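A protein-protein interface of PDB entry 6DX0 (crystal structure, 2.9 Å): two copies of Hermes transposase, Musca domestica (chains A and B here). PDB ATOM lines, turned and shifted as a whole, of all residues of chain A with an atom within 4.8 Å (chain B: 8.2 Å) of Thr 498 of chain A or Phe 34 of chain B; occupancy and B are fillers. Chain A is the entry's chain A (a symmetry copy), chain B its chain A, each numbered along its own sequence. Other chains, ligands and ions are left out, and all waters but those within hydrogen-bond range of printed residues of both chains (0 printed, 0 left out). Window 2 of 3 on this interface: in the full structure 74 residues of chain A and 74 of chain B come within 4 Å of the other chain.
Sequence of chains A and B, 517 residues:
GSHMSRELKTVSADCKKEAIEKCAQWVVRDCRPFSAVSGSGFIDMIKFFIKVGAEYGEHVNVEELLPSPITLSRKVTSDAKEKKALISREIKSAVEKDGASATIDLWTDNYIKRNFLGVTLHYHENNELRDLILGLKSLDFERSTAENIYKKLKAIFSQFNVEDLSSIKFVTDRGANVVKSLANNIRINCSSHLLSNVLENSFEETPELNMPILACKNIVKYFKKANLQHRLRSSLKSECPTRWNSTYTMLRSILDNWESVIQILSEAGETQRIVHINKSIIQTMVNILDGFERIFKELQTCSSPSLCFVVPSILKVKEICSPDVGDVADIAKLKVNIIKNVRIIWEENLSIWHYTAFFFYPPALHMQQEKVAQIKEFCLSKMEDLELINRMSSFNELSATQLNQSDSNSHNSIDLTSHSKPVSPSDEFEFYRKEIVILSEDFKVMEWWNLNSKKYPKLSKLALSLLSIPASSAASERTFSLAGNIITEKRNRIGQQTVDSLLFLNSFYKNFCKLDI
Printed residues of chain A that touch a printed residue of chain B: Pro 69, Leu 72, Ser 73, Val 76, Arg 491, Thr 498 and Leu 502. Hydrophobic or aromatic side chains of chain B within 4 Å of the printed part of chain A: Ala 24, Val 28, Phe 34 and Val 37. Among the printed residues, no Asp or Glu carboxylate lies within 4 Å of a Lys or Arg side-chain nitrogen of the other chain.
No position is printed for both chains.
O of Ser 35 of chain B lies within hydrogen-bond range of OG of Ser 38 of chain B (3.0 Å). N of Arg 32 of chain B sits at hydrogen-bond distance from O of Val 27 of chain B, 3.1 Å away.
Among the printed residues, pairs that only touch across the chains: Pro 69 of chain A with Phe 34 of chain B (3.1 Å), Pro 69 of chain A with Ser 38 of chain B (3.4 Å), Ser 73 of chain A with Phe 34 of chain B (3.4 Å), Thr 498 of chain A with Phe 34 of chain B (3.5 Å), Pro 69 of chain A with Val 37 of chain B (3.6 Å), Leu 502 of chain A with Val 28 of chain B (3.7 Å), Val 76 of chain A with Phe 34 of chain B (3.7 Å), Pro 69 of chain A with Ser 35 of chain B (3.7 Å), Leu 72 of chain A with Val 37 of chain B (3.7 Å), Arg 491 of chain A with Pro 33 of chain B (3.8 Å), Leu 72 of chain A with Cys 23 of chain B (3.8 Å), Val 76 of chain A with Ala 24 of chain B (3.8 Å), Leu 502 of chain A with Phe 34 of chain B (3.9 Å) and Val 76 of chain A with Val 28 of chain B (3.9 Å).
Thr 498 of chain A touches just one residue of chain B: Phe 34. Of chain A, only Pro 69 (3.1 Å), Ser 73 (3.4 Å), Val 76 (3.7 Å), Thr 498 (3.5 Å) and Leu 502 (3.9 Å) come within 4 Å of Phe 34 of chain B. No residue of chain B comes within 4 Å of Gly 495 of chain A. Of the printed residues of chain A, Ala 24 of chain B touches Val 76. Printed residues of chain A within 4 Å of Arg 32 of chain B: Arg 491 (3.5 Å). Of the printed residues of chain B, Arg 491 of chain A touches Arg 32 and Pro 33. Of the printed residues of chain B, Ser 73 of chain A touches Phe 34 (3.4 Å). The nearest residue of chain A that does not touch Phe 34 of chain B is Leu 72 of chain A (4.03 Å). The nearest printed residue of chain A that does not touch Arg 32 of chain B is Leu 502 of chain A (5.8 Å).
The backbone carbonyl oxygen (O) of Arg 32 of chain B sits at hydrogen-bond distance from the guanidinium group (NH1) of Arg 491 of chain A.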
ATOM      1  N   PRO A  69      -3.274   0.643  25.887  1.00  0.00           N
ATOM      2  CA  PRO A  69      -4.432  -0.262  25.855  1.00  0.00           C
ATOM      3  C   PRO A  69      -4.100  -1.656  26.350  1.00  0.00           C
ATOM      4  O   PRO A  69      -4.838  -2.230  27.165  1.00  0.00           O
ATOM      5  CB  PRO A  69      -4.809  -0.258  24.372  1.00  0.00           C
ATOM      6  CG  PRO A  69      -4.352   1.065  23.859  1.00  0.00           C
ATOM      7  CD  PRO A  69      -3.095   1.374  24.617  1.00  0.00           C
ATOM      8  N   LEU A  72      -3.875  -1.377  30.060  1.00  0.00           N
ATOM      9  CA  LEU A  72      -5.275  -1.227  30.465  1.00  0.00           C
ATOM     10  C   LEU A  72      -5.993  -2.571  30.419  1.00  0.00           C
ATOM     11  O   LEU A  72      -6.732  -2.933  31.344  1.00  0.00           O
ATOM     12  CB  LEU A  72      -5.992  -0.212  29.571  1.00  0.00           C
ATOM     13  CG  LEU A  72      -5.679   1.265  29.830  1.00  0.00           C
ATOM     14  CD1 LEU A  72      -6.818   2.180  29.346  1.00  0.00           C
ATOM     15  CD2 LEU A  72      -5.375   1.499  31.309  1.00  0.00           C
ATOM     16  N   SER A  73      -5.768  -3.334  29.345  1.00  0.00           N
ATOM     17  CA  SER A  73      -6.254  -4.706  29.326  1.00  0.00           C
ATOM     18  C   SER A  73      -5.701  -5.498  30.501  1.00  0.00           C
ATOM     19  O   SER A  73      -6.421  -6.290  31.121  1.00  0.00           O
ATOM     20  CB  SER A  73      -5.878  -5.394  28.017  1.00  0.00           C
ATOM     21  OG  SER A  73      -5.993  -6.799  28.174  1.00  0.00           O
ATOM     22  N   VAL A  76      -7.283  -4.321  34.167  1.00  0.00           N
ATOM     23  CA  VAL A  76      -8.627  -4.822  34.457  1.00  0.00           C
ATOM     24  C   VAL A  76      -8.559  -6.296  34.794  1.00  0.00           C
ATOM     25  O   VAL A  76      -9.278  -6.783  35.675  1.00  0.00           O
ATOM     26  CB  VAL A  76      -9.594  -4.563  33.284  1.00  0.00           C
ATOM     27  CG1 VAL A  76      -9.710  -3.099  33.003  1.00  0.00           C
ATOM     28  CG2 VAL A  76      -9.149  -5.289  32.041  1.00  0.00           C
ATOM     29  N   ARG A 491     -14.817  -4.887  18.478  1.00  0.00           N
ATOM     30  CA  ARG A 491     -14.230  -5.470  19.680  1.00  0.00           C
ATOM     31  C   ARG A 491     -14.270  -6.970  19.681  1.00  0.00           C
ATOM     32  O   ARG A 491     -14.111  -7.571  20.748  1.00  0.00           O
ATOM     33  CB  ARG A 491     -14.933  -4.929  20.933  1.00  0.00           C
ATOM     34  CG  ARG A 491     -14.685  -3.423  21.185  1.00  0.00           C
ATOM     35  CD  ARG A 491     -15.120  -2.986  22.586  1.00  0.00           C
ATOM     36  NE  ARG A 491     -14.128  -3.312  23.613  1.00  0.00           N
ATOM     37  CZ  ARG A 491     -14.305  -3.105  24.911  1.00  0.00           C
ATOM     38  NH1 ARG A 491     -15.428  -2.569  25.358  1.00  0.00           N
ATOM     39  NH2 ARG A 491     -13.356  -3.442  25.763  1.00  0.00           N
ATOM     40  N   ILE A 494     -12.325  -9.994  21.575  1.00  0.00           N
ATOM     41  CA  ILE A 494     -12.217  -9.869  23.016  1.00  0.00           C
ATOM     42  C   ILE A 494     -12.205 -11.254  23.641  1.00  0.00           C
ATOM     43  O   ILE A 494     -12.887 -12.175  23.173  1.00  0.00           O
ATOM     44  CB  ILE A 494     -13.350  -8.990  23.569  1.00  0.00           C
ATOM     45  CG1 ILE A 494     -12.926  -8.366  24.906  1.00  0.00           C
ATOM     46  CG2 ILE A 494     -14.601  -9.783  23.750  1.00  0.00           C
ATOM     47  CD1 ILE A 494     -13.247  -6.893  25.007  1.00  0.00           C
ATOM     48  N   GLY A 495     -11.404 -11.407  24.702  1.00  0.00           N
ATOM     49  CA  GLY A 495     -11.213 -12.702  25.316  1.00  0.00           C
ATOM     50  C   GLY A 495     -12.247 -13.008  26.381  1.00  0.00           C
ATOM     51  O   GLY A 495     -12.889 -12.120  26.933  1.00  0.00           O
ATOM     52  N   GLN A 496     -12.412 -14.306  26.645  1.00  0.00           N
ATOM     53  CA  GLN A 496     -13.390 -14.750  27.633  1.00  0.00           C
ATOM     54  C   GLN A 496     -13.091 -14.160  29.003  1.00  0.00           C
ATOM     55  O   GLN A 496     -14.011 -13.805  29.752  1.00  0.00           O
ATOM     56  CB  GLN A 496     -13.399 -16.280  27.706  1.00  0.00           C
ATOM     57  CG  GLN A 496     -13.056 -16.992  26.387  1.00  0.00           C
ATOM     58  CD  GLN A 496     -12.739 -18.472  26.578  1.00  0.00           C
ATOM     59  OE1 GLN A 496     -12.835 -19.001  27.687  1.00  0.00           O
ATOM     60  NE2 GLN A 496     -12.352 -19.143  25.495  1.00  0.00           N
ATOM     61  N   GLN A 497     -11.807 -14.046  29.348  1.00  0.00           N
ATOM     62  CA  GLN A 497     -11.451 -13.519  30.656  1.00  0.00           C
ATOM     63  C   GLN A 497     -11.706 -12.026  30.711  1.00  0.00           C
ATOM     64  O   GLN A 497     -12.294 -11.521  31.672  1.00  0.00           O
ATOM     65  CB  GLN A 497      -9.991 -13.828  30.974  1.00  0.00           C
ATOM     66  CG  GLN A 497      -9.713 -13.875  32.461  1.00  0.00           C
ATOM     67  CD  GLN A 497     -10.743 -14.716  33.205  1.00  0.00           C
ATOM     68  OE1 GLN A 497     -11.014 -15.862  32.838  1.00  0.00           O
ATOM     69  NE2 GLN A 497     -11.334 -14.141  34.245  1.00  0.00           N
ATOM     70  N   THR A 498     -11.275 -11.309  29.678  1.00  0.00           N
ATOM     71  CA  THR A 498     -11.547  -9.884  29.601  1.00  0.00           C
ATOM     72  C   THR A 498     -13.018  -9.578  29.856  1.00  0.00           C
ATOM     73  O   THR A 498     -13.352  -8.599  30.532  1.00  0.00           O
ATOM     74  CB  THR A 498     -11.147  -9.344  28.232  1.00  0.00           C
ATOM     75  OG1 THR A 498      -9.956  -9.998  27.770  1.00  0.00           O
ATOM     76  CG2 THR A 498     -10.924  -7.835  28.331  1.00  0.00           C
ATOM     77  N   VAL A 499     -13.916 -10.408  29.322  1.00  0.00           N
ATOM     78  CA  VAL A 499     -15.341 -10.114  29.434  1.00  0.00           C
ATOM     79  C   VAL A 499     -15.832 -10.392  30.845  1.00  0.00           C
ATOM     80  O   VAL A 499     -16.530  -9.566  31.444  1.00  0.00           O
ATOM     81  CB  VAL A 499     -16.144 -10.909  28.390  1.00  0.00           C
ATOM     82  CG1 VAL A 499     -17.641 -10.706  28.607  1.00  0.00           C
ATOM     83  CG2 VAL A 499     -15.745 -10.481  26.982  1.00  0.00           C
ATOM     84  N   ASP A 500     -15.464 -11.554  31.402  1.00  0.00           N
ATOM     85  CA  ASP A 500     -15.841 -11.867  32.781  1.00  0.00           C
ATOM     86  C   ASP A 500     -15.349 -10.790  33.749  1.00  0.00           C
ATOM     87  O   ASP A 500     -16.074 -10.378  34.665  1.00  0.00           O
ATOM     88  CB  ASP A 500     -15.297 -13.242  33.163  1.00  0.00           C
ATOM     89  CG  ASP A 500     -15.335 -13.499  34.664  1.00  0.00           C
ATOM     90  OD1 ASP A 500     -14.311 -13.236  35.335  1.00  0.00           O
ATOM     91  OD2 ASP A 500     -16.375 -13.975  35.173  1.00  0.00           O
ATOM     92  N   SER A 501     -14.129 -10.303  33.546  1.00  0.00           N
ATOM     93  CA  SER A 501     -13.609  -9.225  34.373  1.00  0.00           C
ATOM     94  C   SER A 501     -14.467  -7.975  34.211  1.00  0.00           C
ATOM     95  O   SER A 501     -15.167  -7.560  35.141  1.00  0.00           O
ATOM     96  CB  SER A 501     -12.156  -8.930  33.996  1.00  0.00           C
ATOM     97  OG  SER A 501     -11.409 -10.126  33.849  1.00  0.00           O
ATOM     98  N   LEU A 502     -14.433  -7.398  33.008  1.00  0.00           N
ATOM     99  CA  LEU A 502     -15.151  -6.164  32.729  1.00  0.00           C
ATOM    100  C   LEU A 502     -16.576  -6.182  33.249  1.00  0.00           C
ATOM    101  O   LEU A 502     -17.109  -5.138  33.631  1.00  0.00           O
ATOM    102  CB  LEU A 502     -15.147  -5.912  31.234  1.00  0.00           C
ATOM    103  CG  LEU A 502     -13.816  -5.426  30.702  1.00  0.00           C
ATOM    104  CD1 LEU A 502     -13.687  -5.659  29.224  1.00  0.00           C
ATOM    105  CD2 LEU A 502     -13.747  -3.954  30.987  1.00  0.00           C
ATOM    106  N   CYS B  23      -7.841   5.153  34.552  1.00  0.00           N
ATOM    107  CA  CYS B  23      -8.235   4.843  33.187  1.00  0.00           C
ATOM    108  C   CYS B  23      -8.984   3.515  33.115  1.00  0.00           C
ATOM    109  O   CYS B  23     -10.031   3.411  32.461  1.00  0.00           O
ATOM    110  CB  CYS B  23      -6.999   4.827  32.300  1.00  0.00           C
ATOM    111  SG  CYS B  23      -6.445   6.470  31.942  1.00  0.00           S
ATOM    112  N   ALA B  24      -8.464   2.484  33.781  1.00  0.00           N
ATOM    113  CA  ALA B  24      -9.175   1.215  33.841  1.00  0.00           C
ATOM    114  C   ALA B  24     -10.504   1.326  34.570  1.00  0.00           C
ATOM    115  O   ALA B  24     -11.289   0.376  34.532  1.00  0.00           O
ATOM    116  CB  ALA B  24      -8.305   0.148  34.504  1.00  0.00           C
ATOM    117  N   TRP B  26     -12.486   4.161  33.946  1.00  0.00           N
ATOM    118  CA  TRP B  26     -13.259   4.751  32.869  1.00  0.00           C
ATOM    119  C   TRP B  26     -13.844   3.677  31.975  1.00  0.00           C
ATOM    120  O   TRP B  26     -15.006   3.750  31.560  1.00  0.00           O
ATOM    121  CB  TRP B  26     -12.349   5.647  32.059  1.00  0.00           C
ATOM    122  CG  TRP B  26     -12.961   6.237  30.885  1.00  0.00           C
ATOM    123  CD1 TRP B  26     -14.213   6.758  30.782  1.00  0.00           C
ATOM    124  CD2 TRP B  26     -12.340   6.411  29.618  1.00  0.00           C
ATOM    125  NE1 TRP B  26     -14.412   7.248  29.516  1.00  0.00           N
ATOM    126  CE2 TRP B  26     -13.270   7.047  28.784  1.00  0.00           C
ATOM    127  CE3 TRP B  26     -11.084   6.094  29.109  1.00  0.00           C
ATOM    128  CZ2 TRP B  26     -12.984   7.374  27.469  1.00  0.00           C
ATOM    129  CZ3 TRP B  26     -10.804   6.407  27.803  1.00  0.00           C
ATOM    130  CH2 TRP B  26     -11.746   7.047  26.997  1.00  0.00           C
ATOM    131  N   VAL B  27     -13.047   2.658  31.689  1.00  0.00           N
ATOM    132  CA  VAL B  27     -13.398   1.678  30.681  1.00  0.00           C
ATOM    133  C   VAL B  27     -14.400   0.647  31.204  1.00  0.00           C
ATOM    134  O   VAL B  27     -15.244   0.158  30.445  1.00  0.00           O
ATOM    135  CB  VAL B  27     -12.086   1.059  30.178  1.00  0.00           C
ATOM    136  CG1 VAL B  27     -12.263  -0.406  29.808  1.00  0.00           C
ATOM    137  CG2 VAL B  27     -11.540   1.903  29.019  1.00  0.00           C
ATOM    138  N   VAL B  28     -14.363   0.312  32.487  1.00  0.00           N
ATOM    139  CA  VAL B  28     -15.336  -0.656  32.974  1.00  0.00           C
ATOM    140  C   VAL B  28     -16.655   0.029  33.314  1.00  0.00           C
ATOM    141  O   VAL B  28     -17.734  -0.510  33.048  1.00  0.00           O
ATOM    142  CB  VAL B  28     -14.763  -1.454  34.168  1.00  0.00           C
ATOM    143  CG1 VAL B  28     -13.301  -1.811  33.927  1.00  0.00           C
ATOM    144  CG2 VAL B  28     -14.904  -0.709  35.453  1.00  0.00           C
ATOM    145  N   CYS B  31     -18.113   1.319  29.869  1.00  0.00           N
ATOM    146  CA  CYS B  31     -18.051   0.307  28.804  1.00  0.00           C
ATOM    147  C   CYS B  31     -17.407   0.853  27.526  1.00  0.00           C
ATOM    148  O   CYS B  31     -18.034   0.955  26.473  1.00  0.00           O
ATOM    149  CB  CYS B  31     -19.445  -0.257  28.502  1.00  0.00           C
ATOM    150  SG  CYS B  31     -19.924  -1.736  29.444  1.00  0.00           S
ATOM    151  N   ARG B  32     -16.132   1.197  27.622  1.00  0.00           N
ATOM    152  CA  ARG B  32     -15.435   1.797  26.495  1.00  0.00           C
ATOM    153  C   ARG B  32     -14.263   0.936  26.036  1.00  0.00           C
ATOM    154  O   ARG B  32     -13.740   0.121  26.804  1.00  0.00           O
ATOM    155  CB  ARG B  32     -14.932   3.201  26.860  1.00  0.00           C
ATOM    156  CG  ARG B  32     -16.027   4.167  27.294  1.00  0.00           C
ATOM    157  CD  ARG B  32     -16.425   5.100  26.189  1.00  0.00           C
ATOM    158  NE  ARG B  32     -17.458   6.023  26.642  1.00  0.00           N
ATOM    159  CZ  ARG B  32     -18.755   5.739  26.679  1.00  0.00           C
ATOM    160  NH1 ARG B  32     -19.184   4.554  26.286  1.00  0.00           N
ATOM    161  NH2 ARG B  32     -19.626   6.638  27.114  1.00  0.00           N
ATOM    162  N   PRO B  33     -13.830   1.085  24.787  1.00  0.00           N
ATOM    163  CA  PRO B  33     -12.693   0.290  24.299  1.00  0.00           C
ATOM    164  C   PRO B  33     -11.368   0.634  24.973  1.00  0.00           C
ATOM    165  O   PRO B  33     -11.031   1.800  25.191  1.00  0.00           O
ATOM    166  CB  PRO B  33     -12.645   0.614  22.797  1.00  0.00           C
ATOM    167  CG  PRO B  33     -13.484   1.844  22.622  1.00  0.00           C
ATOM    168  CD  PRO B  33     -14.532   1.767  23.690  1.00  0.00           C
ATOM    169  N   PHE B  34     -10.601  -0.420  25.261  1.00  0.00           N
ATOM    170  CA  PHE B  34      -9.228  -0.331  25.741  1.00  0.00           C
ATOM    171  C   PHE B  34      -8.359   0.632  24.955  1.00  0.00           C
ATOM    172  O   PHE B  34      -7.362   1.124  25.490  1.00  0.00           O
ATOM    173  CB  PHE B  34      -8.570  -1.706  25.667  1.00  0.00           C
ATOM    174  CG  PHE B  34      -9.089  -2.677  26.673  1.00  0.00           C
ATOM    175  CD1 PHE B  34      -8.780  -4.013  26.576  1.00  0.00           C
ATOM    176  CD2 PHE B  34      -9.878  -2.246  27.727  1.00  0.00           C
ATOM    177  CE1 PHE B  34      -9.249  -4.910  27.508  1.00  0.00           C
ATOM    178  CE2 PHE B  34     -10.343  -3.138  28.667  1.00  0.00           C
ATOM    179  CZ  PHE B  34     -10.029  -4.467  28.561  1.00  0.00           C
ATOM    180  N   SER B  35      -8.681   0.878  23.697  1.00  0.00           N
ATOM    181  CA  SER B  35      -7.854   1.699  22.838  1.00  0.00           C
ATOM    182  C   SER B  35      -8.426   3.081  22.666  1.00  0.00           C
ATOM    183  O   SER B  35      -8.052   3.785  21.721  1.00  0.00           O
ATOM    184  CB  SER B  35      -7.704   1.037  21.477  1.00  0.00           C
ATOM    185  OG  SER B  35      -8.980   0.614  21.037  1.00  0.00           O
ATOM    186  N   ALA B  36      -9.383   3.456  23.510  1.00  0.00           N
ATOM    187  CA  ALA B  36      -9.747   4.861  23.582  1.00  0.00           C
ATOM    188  C   ALA B  36      -8.591   5.676  24.149  1.00  0.00           C
ATOM    189  O   ALA B  36      -8.312   6.784  23.686  1.00  0.00           O
ATOM    190  CB  ALA B  36     -11.014   5.018  24.419  1.00  0.00           C
ATOM    191  N   VAL B  37      -7.864   5.101  25.110  1.00  0.00           N
ATOM    192  CA  VAL B  37      -6.699   5.734  25.709  1.00  0.00           C
ATOM    193  C   VAL B  37      -5.631   6.096  24.686  1.00  0.00           C
ATOM    194  O   VAL B  37      -4.787   6.963  24.949  1.00  0.00           O
ATOM    195  CB  VAL B  37      -6.119   4.789  26.780  1.00  0.00           C
ATOM    196  CG1 VAL B  37      -5.605   3.532  26.117  1.00  0.00           C
ATOM    197  CG2 VAL B  37      -5.017   5.483  27.588  1.00  0.00           C
ATOM    198  N   SER B  38      -5.623   5.446  23.529  1.00  0.00           N
ATOM    199  CA  SER B  38      -4.557   5.666  22.567  1.00  0.00           C
ATOM    200  C   SER B  38      -4.994   6.553  21.417  1.00  0.00           C
ATOM    201  O   SER B  38      -4.295   6.628  20.401  1.00  0.00           O
ATOM    202  CB  SER B  38      -4.020   4.327  22.043  1.00  0.00           C
ATOM    203  OG  SER B  38      -5.043   3.453  21.589  1.00  0.00           O
ATOM    204  N   GLY B  39      -6.117   7.252  21.565  1.00  0.00           N
ATOM    205  CA  GLY B  39      -6.710   7.978  20.451  1.00  0.00           C
ATOM    206  C   GLY B  39      -6.171   9.388  20.294  1.00  0.00           C
ATOM    207  O   GLY B  39      -6.165  10.172  21.247  1.00  0.00           O
